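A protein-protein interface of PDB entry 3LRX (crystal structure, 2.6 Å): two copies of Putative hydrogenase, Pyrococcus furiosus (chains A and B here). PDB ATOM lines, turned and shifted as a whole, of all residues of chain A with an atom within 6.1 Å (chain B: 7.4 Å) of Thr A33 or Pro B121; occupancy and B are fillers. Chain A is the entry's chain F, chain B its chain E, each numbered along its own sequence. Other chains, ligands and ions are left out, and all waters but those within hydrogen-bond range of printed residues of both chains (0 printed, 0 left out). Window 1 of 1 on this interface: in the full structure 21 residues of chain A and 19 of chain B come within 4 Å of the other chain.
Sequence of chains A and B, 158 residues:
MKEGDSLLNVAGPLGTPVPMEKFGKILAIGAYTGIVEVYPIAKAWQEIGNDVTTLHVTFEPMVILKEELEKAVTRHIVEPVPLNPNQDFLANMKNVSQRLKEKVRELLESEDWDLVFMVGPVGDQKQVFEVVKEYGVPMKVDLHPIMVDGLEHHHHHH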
ATOM      1  N   GLY A  30     -14.010  -5.341  21.060  1.00  0.00           N
ATOM      2  CA  GLY A  30     -14.731  -6.331  20.286  1.00  0.00           C
ATOM      3  C   GLY A  30     -16.218  -6.340  20.602  1.00  0.00           C
ATOM      4  O   GLY A  30     -16.622  -6.728  21.696  1.00  0.00           O
ATOM      5  N   ALA A  31     -17.045  -5.924  19.651  1.00  0.00           N
ATOM      6  CA  ALA A  31     -18.482  -5.894  19.875  1.00  0.00           C
ATOM      7  C   ALA A  31     -19.112  -7.161  19.331  1.00  0.00           C
ATOM      8  O   ALA A  31     -18.841  -7.566  18.203  1.00  0.00           O
ATOM      9  CB  ALA A  31     -19.088  -4.674  19.202  1.00  0.00           C
ATOM     10  N   TYR A  32     -19.959  -7.792  20.135  1.00  0.00           N
ATOM     11  CA  TYR A  32     -20.621  -9.033  19.733  1.00  0.00           C
ATOM     12  C   TYR A  32     -19.613 -10.096  19.317  1.00  0.00           C
ATOM     13  O   TYR A  32     -18.630 -10.361  20.012  1.00  0.00           O
ATOM     14  CB  TYR A  32     -21.585  -8.777  18.575  1.00  0.00           C
ATOM     15  CG  TYR A  32     -22.607  -7.703  18.851  1.00  0.00           C
ATOM     16  CD1 TYR A  32     -22.460  -6.423  18.327  1.00  0.00           C
ATOM     17  CD2 TYR A  32     -23.709  -7.952  19.665  1.00  0.00           C
ATOM     18  CE1 TYR A  32     -23.386  -5.416  18.605  1.00  0.00           C
ATOM     19  CE2 TYR A  32     -24.637  -6.945  19.951  1.00  0.00           C
ATOM     20  CZ  TYR A  32     -24.466  -5.684  19.417  1.00  0.00           C
ATOM     21  OH  TYR A  32     -25.367  -4.688  19.698  1.00  0.00           O
ATOM     22  N   THR A  33     -19.861 -10.706  18.171  1.00  0.00           N
ATOM     23  CA  THR A  33     -18.979 -11.747  17.681  1.00  0.00           C
ATOM     24  C   THR A  33     -17.602 -11.227  17.281  1.00  0.00           C
ATOM     25  O   THR A  33     -16.650 -11.992  17.151  1.00  0.00           O
ATOM     26  CB  THR A  33     -19.627 -12.478  16.488  1.00  0.00           C
ATOM     27  OG1 THR A  33     -19.970 -11.533  15.472  1.00  0.00           O
ATOM     28  CG2 THR A  33     -20.889 -13.195  16.931  1.00  0.00           C
ATOM     29  N   GLY A  34     -17.493  -9.919  17.092  1.00  0.00           N
ATOM     30  CA  GLY A  34     -16.217  -9.349  16.704  1.00  0.00           C
ATOM     31  C   GLY A  34     -15.057  -9.717  17.621  1.00  0.00           C
ATOM     32  O   GLY A  34     -13.907  -9.753  17.196  1.00  0.00           O
ATOM     33  N   ILE A  35     -15.344  -9.998  18.883  1.00  0.00           N
ATOM     34  CA  ILE A  35     -14.288 -10.338  19.815  1.00  0.00           C
ATOM     35  C   ILE A  35     -13.468 -11.538  19.343  1.00  0.00           C
ATOM     36  O   ILE A  35     -12.286 -11.655  19.656  1.00  0.00           O
ATOM     37  CB  ILE A  35     -14.876 -10.642  21.209  1.00  0.00           C
ATOM     38  CG1 ILE A  35     -13.761 -10.662  22.252  1.00  0.00           C
ATOM     39  CG2 ILE A  35     -15.611 -11.979  21.192  1.00  0.00           C
ATOM     40  CD1 ILE A  35     -13.129  -9.327  22.459  1.00  0.00           C
ATOM     41  N   VAL A  36     -14.088 -12.438  18.591  1.00  0.00           N
ATOM     42  CA  VAL A  36     -13.381 -13.617  18.117  1.00  0.00           C
ATOM     43  C   VAL A  36     -12.207 -13.244  17.234  1.00  0.00           C
ATOM     44  O   VAL A  36     -11.111 -13.792  17.355  1.00  0.00           O
ATOM     45  CB  VAL A  36     -14.314 -14.526  17.335  1.00  0.00           C
ATOM     46  CG1 VAL A  36     -13.540 -15.701  16.763  1.00  0.00           C
ATOM     47  CG2 VAL A  36     -15.416 -15.002  18.244  1.00  0.00           C
ATOM     48  N   GLU A  37     -12.441 -12.309  16.333  1.00  0.00           N
ATOM     49  CA  GLU A  37     -11.391 -11.865  15.431  1.00  0.00           C
ATOM     50  C   GLU A  37     -10.305 -11.048  16.153  1.00  0.00           C
ATOM     51  O   GLU A  37      -9.133 -11.094  15.769  1.00  0.00           O
ATOM     52  CB  GLU A  37     -12.014 -11.038  14.312  1.00  0.00           C
ATOM     53  CG  GLU A  37     -11.032 -10.514  13.298  1.00  0.00           C
ATOM     54  CD  GLU A  37     -11.709  -9.754  12.174  1.00  0.00           C
ATOM     55  OE1 GLU A  37     -10.973  -9.231  11.302  1.00  0.00           O
ATOM     56  OE2 GLU A  37     -12.967  -9.680  12.158  1.00  0.00           O
ATOM     57  N   HIS A  56     -14.820  -6.503  25.617  1.00  0.00           N
ATOM     58  CA  HIS A  56     -15.862  -7.238  24.903  1.00  0.00           C
ATOM     59  C   HIS A  56     -17.218  -6.733  25.373  1.00  0.00           C
ATOM     60  O   HIS A  56     -17.563  -6.882  26.540  1.00  0.00           O
ATOM     61  CB  HIS A  56     -15.759  -8.737  25.200  1.00  0.00           C
ATOM     62  CG  HIS A  56     -16.727  -9.572  24.432  1.00  0.00           C
ATOM     63  ND1 HIS A  56     -17.031 -10.869  24.784  1.00  0.00           N
ATOM     64  CD2 HIS A  56     -17.439  -9.303  23.313  1.00  0.00           C
ATOM     65  CE1 HIS A  56     -17.891 -11.364  23.911  1.00  0.00           C
ATOM     66  NE2 HIS A  56     -18.155 -10.434  23.011  1.00  0.00           N
ATOM     67  N   THR A  58     -21.034  -7.306  24.602  1.00  0.00           N
ATOM     68  CA  THR A  58     -22.051  -8.076  23.900  1.00  0.00           C
ATOM     69  C   THR A  58     -23.235  -8.313  24.845  1.00  0.00           C
ATOM     70  O   THR A  58     -23.346  -7.660  25.893  1.00  0.00           O
ATOM     71  CB  THR A  58     -21.456  -9.434  23.434  1.00  0.00           C
ATOM     72  OG1 THR A  58     -22.439 -10.170  22.708  1.00  0.00           O
ATOM     73  CG2 THR A  58     -21.005 -10.265  24.627  1.00  0.00           C
ATOM     74  N   MET A  62     -23.869 -14.123  25.551  1.00  0.00           N
ATOM     75  CA  MET A  62     -22.995 -14.244  24.390  1.00  0.00           C
ATOM     76  C   MET A  62     -21.526 -14.037  24.695  1.00  0.00           C
ATOM     77  O   MET A  62     -20.709 -14.018  23.778  1.00  0.00           O
ATOM     78  CB  MET A  62     -23.417 -13.258  23.301  1.00  0.00           C
ATOM     79  CG  MET A  62     -24.908 -13.035  23.221  1.00  0.00           C
ATOM     80  SD  MET A  62     -25.571 -12.806  21.431  1.00  0.00           S
ATOM     81  CE  MET A  62     -24.177 -11.678  20.684  1.00  0.00           C
ATOM     82  N   VAL A 119     -13.353  -3.970  16.135  1.00  0.00           N
ATOM     83  CA  VAL A 119     -13.943  -4.839  15.131  1.00  0.00           C
ATOM     84  C   VAL A 119     -15.361  -5.059  15.641  1.00  0.00           C
ATOM     85  O   VAL A 119     -15.569  -5.560  16.749  1.00  0.00           O
ATOM     86  CB  VAL A 119     -13.183  -6.191  15.024  1.00  0.00           C
ATOM     87  CG1 VAL A 119     -12.845  -6.679  16.407  1.00  0.00           C
ATOM     88  CG2 VAL A 119     -14.024  -7.230  14.318  1.00  0.00           C
ATOM     89  N   GLY B  30     -26.145 -11.737   5.153  1.00  0.00           N
ATOM     90  CA  GLY B  30     -25.908 -10.971   6.358  1.00  0.00           C
ATOM     91  C   GLY B  30     -25.989 -11.830   7.613  1.00  0.00           C
ATOM     92  O   GLY B  30     -27.070 -12.298   7.991  1.00  0.00           O
ATOM     93  N   ALA B  31     -24.852 -12.040   8.271  1.00  0.00           N
ATOM     94  CA  ALA B  31     -24.836 -12.844   9.481  1.00  0.00           C
ATOM     95  C   ALA B  31     -24.962 -11.944  10.706  1.00  0.00           C
ATOM     96  O   ALA B  31     -24.257 -10.943  10.829  1.00  0.00           O
ATOM     97  CB  ALA B  31     -23.549 -13.663   9.539  1.00  0.00           C
ATOM     98  N   TYR B  32     -25.862 -12.299  11.614  1.00  0.00           N
ATOM     99  CA  TYR B  32     -26.073 -11.510  12.829  1.00  0.00           C
ATOM    100  C   TYR B  32     -26.384 -10.061  12.508  1.00  0.00           C
ATOM    101  O   TYR B  32     -27.219  -9.776  11.662  1.00  0.00           O
ATOM    102  CB  TYR B  32     -24.842 -11.572  13.748  1.00  0.00           C
ATOM    103  CG  TYR B  32     -24.387 -12.970  14.096  1.00  0.00           C
ATOM    104  CD1 TYR B  32     -23.302 -13.554  13.450  1.00  0.00           C
ATOM    105  CD2 TYR B  32     -25.060 -13.721  15.046  1.00  0.00           C
ATOM    106  CE1 TYR B  32     -22.897 -14.859  13.744  1.00  0.00           C
ATOM    107  CE2 TYR B  32     -24.667 -15.027  15.348  1.00  0.00           C
ATOM    108  CZ  TYR B  32     -23.585 -15.587  14.692  1.00  0.00           C
ATOM    109  OH  TYR B  32     -23.181 -16.870  14.984  1.00  0.00           O
ATOM    110  N   THR B  33     -25.705  -9.145  13.178  1.00  0.00           N
ATOM    111  CA  THR B  33     -25.943  -7.724  12.962  1.00  0.00           C
ATOM    112  C   THR B  33     -25.497  -7.261  11.583  1.00  0.00           C
ATOM    113  O   THR B  33     -25.904  -6.201  11.120  1.00  0.00           O
ATOM    114  CB  THR B  33     -25.222  -6.890  14.035  1.00  0.00           C
ATOM    115  OG1 THR B  33     -23.831  -7.244  14.054  1.00  0.00           O
ATOM    116  CG2 THR B  33     -25.822  -7.168  15.409  1.00  0.00           C
ATOM    117  N   GLY B  34     -24.675  -8.061  10.921  1.00  0.00           N
ATOM    118  CA  GLY B  34     -24.209  -7.683   9.600  1.00  0.00           C
ATOM    119  C   GLY B  34     -25.310  -7.353   8.616  1.00  0.00           C
ATOM    120  O   GLY B  34     -25.095  -6.612   7.662  1.00  0.00           O
ATOM    121  N   PHE B  59     -29.734 -15.417  15.294  1.00  0.00           N
ATOM    122  CA  PHE B  59     -30.452 -16.151  16.332  1.00  0.00           C
ATOM    123  C   PHE B  59     -31.914 -15.731  16.287  1.00  0.00           C
ATOM    124  O   PHE B  59     -32.205 -14.584  15.975  1.00  0.00           O
ATOM    125  CB  PHE B  59     -29.855 -15.861  17.718  1.00  0.00           C
ATOM    126  CG  PHE B  59     -28.525 -16.529  17.959  1.00  0.00           C
ATOM    127  CD1 PHE B  59     -28.398 -17.914  17.842  1.00  0.00           C
ATOM    128  CD2 PHE B  59     -27.396 -15.777  18.274  1.00  0.00           C
ATOM    129  CE1 PHE B  59     -27.165 -18.546  18.028  1.00  0.00           C
ATOM    130  CE2 PHE B  59     -26.162 -16.400  18.460  1.00  0.00           C
ATOM    131  CZ  PHE B  59     -26.046 -17.791  18.337  1.00  0.00           C
ATOM    132  N   MET B  62     -33.203 -12.291  17.185  1.00  0.00           N
ATOM    133  CA  MET B  62     -32.387 -11.208  16.638  1.00  0.00           C
ATOM    134  C   MET B  62     -32.734 -10.819  15.213  1.00  0.00           C
ATOM    135  O   MET B  62     -32.059  -9.980  14.626  1.00  0.00           O
ATOM    136  CB  MET B  62     -30.901 -11.579  16.695  1.00  0.00           C
ATOM    137  CG  MET B  62     -30.518 -12.410  17.893  1.00  0.00           C
ATOM    138  SD  MET B  62     -28.846 -11.878  18.634  1.00  0.00           S
ATOM    139  CE  MET B  62     -27.782 -11.772  17.022  1.00  0.00           C
ATOM    140  N   PHE B  89     -21.999 -20.177  24.302  1.00  0.00           N
ATOM    141  CA  PHE B  89     -22.086 -19.372  23.090  1.00  0.00           C
ATOM    142  C   PHE B  89     -21.265 -19.888  21.910  1.00  0.00           C
ATOM    143  O   PHE B  89     -21.754 -19.928  20.779  1.00  0.00           O
ATOM    144  CB  PHE B  89     -21.699 -17.931  23.403  1.00  0.00           C
ATOM    145  CG  PHE B  89     -22.156 -16.953  22.373  1.00  0.00           C
ATOM    146  CD1 PHE B  89     -21.236 -16.169  21.690  1.00  0.00           C
ATOM    147  CD2 PHE B  89     -23.512 -16.793  22.105  1.00  0.00           C
ATOM    148  CE1 PHE B  89     -21.655 -15.235  20.750  1.00  0.00           C
ATOM    149  CE2 PHE B  89     -23.950 -15.863  21.169  1.00  0.00           C
ATOM    150  CZ  PHE B  89     -23.017 -15.079  20.489  1.00  0.00           C
ATOM    151  N   MET B  93     -22.699 -20.457  18.246  1.00  0.00           N
ATOM    152  CA  MET B  93     -22.223 -19.779  17.055  1.00  0.00           C
ATOM    153  C   MET B  93     -21.896 -20.799  15.980  1.00  0.00           C
ATOM    154  O   MET B  93     -21.972 -20.510  14.785  1.00  0.00           O
ATOM    155  CB  MET B  93     -20.981 -18.960  17.374  1.00  0.00           C
ATOM    156  CG  MET B  93     -21.268 -17.610  18.005  1.00  0.00           C
ATOM    157  SD  MET B  93     -19.618 -16.606  18.190  1.00  0.00           S
ATOM    158  CE  MET B  93     -19.003 -16.682  16.357  1.00  0.00           C
ATOM    159  N   SER B  97     -22.955 -21.170  12.027  1.00  0.00           N
ATOM    160  CA  SER B  97     -21.956 -21.519  11.027  1.00  0.00           C
ATOM    161  C   SER B  97     -22.443 -22.697  10.202  1.00  0.00           C
ATOM    162  O   SER B  97     -22.100 -22.825   9.028  1.00  0.00           O
ATOM    163  CB  SER B  97     -20.636 -21.915  11.683  1.00  0.00           C
ATOM    164  OG  SER B  97     -20.006 -20.819  12.299  1.00  0.00           O
ATOM    165  N   LEU B 100     -25.630 -21.575   8.136  1.00  0.00           N
ATOM    166  CA  LEU B 100     -25.067 -20.693   7.130  1.00  0.00           C
ATOM    167  C   LEU B 100     -24.444 -21.451   5.952  1.00  0.00           C
ATOM    168  O   LEU B 100     -24.742 -21.150   4.798  1.00  0.00           O
ATOM    169  CB  LEU B 100     -24.040 -19.758   7.775  1.00  0.00           C
ATOM    170  CG  LEU B 100     -23.393 -18.712   6.865  1.00  0.00           C
ATOM    171  CD1 LEU B 100     -24.455 -17.881   6.189  1.00  0.00           C
ATOM    172  CD2 LEU B 100     -22.472 -17.844   7.686  1.00  0.00           C
ATOM    173  N   MET B 118     -21.329 -10.589   1.177  1.00  0.00           N
ATOM    174  CA  MET B 118     -21.593 -10.963   2.555  1.00  0.00           C
ATOM    175  C   MET B 118     -20.870 -10.094   3.573  1.00  0.00           C
ATOM    176  O   MET B 118     -19.762  -9.622   3.334  1.00  0.00           O
ATOM    177  CB  MET B 118     -21.188 -12.420   2.785  1.00  0.00           C
ATOM    178  CG  MET B 118     -21.524 -12.912   4.182  1.00  0.00           C
ATOM    179  SD  MET B 118     -20.645 -14.548   4.670  1.00  0.00           S
ATOM    180  CE  MET B 118     -20.762 -14.372   6.612  1.00  0.00           C
ATOM    181  N   VAL B 119     -21.499  -9.895   4.720  1.00  0.00           N
ATOM    182  CA  VAL B 119     -20.873  -9.118   5.774  1.00  0.00           C
ATOM    183  C   VAL B 119     -21.214  -9.775   7.104  1.00  0.00           C
ATOM    184  O   VAL B 119     -22.348  -9.730   7.574  1.00  0.00           O
ATOM    185  CB  VAL B 119     -21.308  -7.616   5.723  1.00  0.00           C
ATOM    186  CG1 VAL B 119     -22.784  -7.497   5.374  1.00  0.00           C
ATOM    187  CG2 VAL B 119     -21.012  -6.939   7.053  1.00  0.00           C
ATOM    188  N   GLY B 120     -20.223 -10.440   7.680  1.00  0.00           N
ATOM    189  CA  GLY B 120     -20.428 -11.112   8.945  1.00  0.00           C
ATOM    190  C   GLY B 120     -19.055 -11.320   9.525  1.00  0.00           C
ATOM    191  O   GLY B 120     -18.093 -10.831   8.949  1.00  0.00           O
ATOM    192  N   PRO B 121     -18.924 -12.011  10.665  1.00  0.00           N
ATOM    193  CA  PRO B 121     -17.604 -12.236  11.252  1.00  0.00           C
ATOM    194  C   PRO B 121     -16.701 -13.051  10.335  1.00  0.00           C
ATOM    195  O   PRO B 121     -17.129 -13.987   9.649  1.00  0.00           O
ATOM    196  CB  PRO B 121     -17.925 -12.945  12.564  1.00  0.00           C
ATOM    197  CG  PRO B 121     -19.243 -13.603  12.292  1.00  0.00           C
ATOM    198  CD  PRO B 121     -19.980 -12.540  11.541  1.00  0.00           C
ATOM    199  N   VAL B 122     -15.436 -12.667  10.335  1.00  0.00           N
ATOM    200  CA  VAL B 122     -14.432 -13.307   9.513  1.00  0.00           C
ATOM    201  C   VAL B 122     -14.513 -14.831   9.486  1.00  0.00           C
ATOM    202  O   VAL B 122     -14.301 -15.444   8.441  1.00  0.00           O
ATOM    203  CB  VAL B 122     -13.025 -12.873   9.968  1.00  0.00           C
ATOM    204  CG1 VAL B 122     -11.956 -13.593   9.151  1.00  0.00           C
ATOM    205  CG2 VAL B 122     -12.887 -11.369   9.791  1.00  0.00           C
ATOM    206  N   GLY B 123     -14.810 -15.430  10.632  1.00  0.00           N
ATOM    207  CA  GLY B 123     -14.899 -16.872  10.708  1.00  0.00           C
ATOM    208  C   GLY B 123     -15.978 -17.418   9.808  1.00  0.00           C
ATOM    209  O   GLY B 123     -15.792 -18.425   9.134  1.00  0.00           O
ATOM    210  N   ASP B 124     -17.119 -16.747   9.786  1.00  0.00           N
ATOM    211  CA  ASP B 124     -18.197 -17.219   8.949  1.00  0.00           C
ATOM    212  C   ASP B 124     -17.979 -16.888   7.499  1.00  0.00           C
ATOM    213  O   ASP B 124     -18.518 -17.564   6.621  1.00  0.00           O
ATOM    214  CB  ASP B 124     -19.521 -16.664   9.441  1.00  0.00           C
ATOM    215  CG  ASP B 124     -19.939 -17.294  10.742  1.00  0.00           C
ATOM    216  OD1 ASP B 124     -19.893 -18.540  10.809  1.00  0.00           O
ATOM    217  OD2 ASP B 124     -20.308 -16.564  11.689  1.00  0.00           O
ATOM    218  N   GLN B 125     -17.185 -15.862   7.226  1.00  0.00           N
ATOM    219  CA  GLN B 125     -16.935 -15.509   5.834  1.00  0.00           C
ATOM    220  C   GLN B 125     -16.059 -16.551   5.157  1.00  0.00           C
ATOM    221  O   GLN B 125     -16.297 -16.941   4.003  1.00  0.00           O
ATOM    222  CB  GLN B 125     -16.244 -14.165   5.733  1.00  0.00           C
ATOM    223  CG  GLN B 125     -16.878 -13.132   6.578  1.00  0.00           C
ATOM    224  CD  GLN B 125     -16.525 -11.756   6.123  1.00  0.00           C
ATOM    225  OE1 GLN B 125     -16.932 -11.324   5.051  1.00  0.00           O
ATOM    226  NE2 GLN B 125     -15.759 -11.052   6.931  1.00  0.00           N
ATOM    227  N   LYS B 126     -15.033 -16.984   5.880  1.00  0.00           N
ATOM    228  CA  LYS B 126     -14.120 -17.978   5.354  1.00  0.00           C
ATOM    229  C   LYS B 126     -14.903 -19.250   5.071  1.00  0.00           C
ATOM    230  O   LYS B 126     -14.746 -19.862   4.018  1.00  0.00           O
ATOM    231  CB  LYS B 126     -12.985 -18.240   6.349  1.00  0.00           C
ATOM    232  CG  LYS B 126     -12.024 -17.077   6.466  1.00  0.00           C
ATOM    233  CD  LYS B 126     -10.664 -17.495   7.005  1.00  0.00           C
ATOM    234  CE  LYS B 126     -10.764 -18.080   8.399  1.00  0.00           C
ATOM    235  NZ  LYS B 126      -9.436 -18.507   8.927  1.00  0.00           N
ATOM    236  N   GLN B 127     -15.772 -19.615   6.004  1.00  0.00           N
ATOM    237  CA  GLN B 127     -16.595 -20.807   5.866  1.00  0.00           C
ATOM    238  C   GLN B 127     -17.490 -20.755   4.619  1.00  0.00           C
ATOM    239  O   GLN B 127     -17.598 -21.742   3.893  1.00  0.00           O
ATOM    240  CB  GLN B 127     -17.450 -20.984   7.126  1.00  0.00           C
ATOM    241  CG  GLN B 127     -16.640 -21.226   8.402  1.00  0.00           C
ATOM    242  CD  GLN B 127     -16.036 -22.624   8.458  1.00  0.00           C
ATOM    243  OE1 GLN B 127     -16.745 -23.607   8.683  1.00  0.00           O
ATOM    244  NE2 GLN B 127     -14.722 -22.719   8.241  1.00  0.00           N
ATOM    245  N   ASP B 142     -16.886  -7.879   3.286  1.00  0.00           N
ATOM    246  CA  ASP B 142     -17.030  -6.528   3.828  1.00  0.00           C
ATOM    247  C   ASP B 142     -15.691  -5.802   3.957  1.00  0.00           C
ATOM    248  O   ASP B 142     -14.631  -6.432   3.997  1.00  0.00           O
ATOM    249  CB  ASP B 142     -17.738  -6.574   5.199  1.00  0.00           C
ATOM    250  CG  ASP B 142     -16.871  -7.175   6.301  1.00  0.00           C
ATOM    251  OD1 ASP B 142     -15.809  -6.594   6.618  1.00  0.00           O
ATOM    252  OD2 ASP B 142     -17.260  -8.219   6.864  1.00  0.00           O
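The side-chain hydroxyl (OG) of Ser B97 is in hydrogen-bond range of the backbone carbonyl oxygen (O) of Met B93, 3.2 Å away.
CG2 of Thr A33 touches SD of Met B93, 3.9 Å away.
Pro B121 touches Thr A33.
Val B122 touches Glu A37.
O of Met A62 touches CD1 of Phe B89 (3.0 Å).
Thr A33 touches just these residues of chain B: Met B93 (3.9 Å) and Pro B121 (3.8 Å).
Of the printed residues of chain B, Glu A37 touches Val B122 (2.9 Å).
Of the printed residues of chain B, Met A62 touches Phe B89.
Of the printed residues of chain A, Phe B89 touches Met A62 (3.0 Å).
Printed residues of chain A within 4 Å of Pro B121: Thr A33 (3.8 Å).
Of the printed residues of chain A, Val B122 touches Glu A37 (2.9 Å).
The nearest residue of chain B that does not touch Thr A33 is Tyr B32 (4.1 Å).
Printed residues of chain A that touch a printed residue of chain B: Thr A33, Glu A37 and Met A62.
Positions printed for both chains: 30, 31, 32, 33, 34, 62 and 119.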
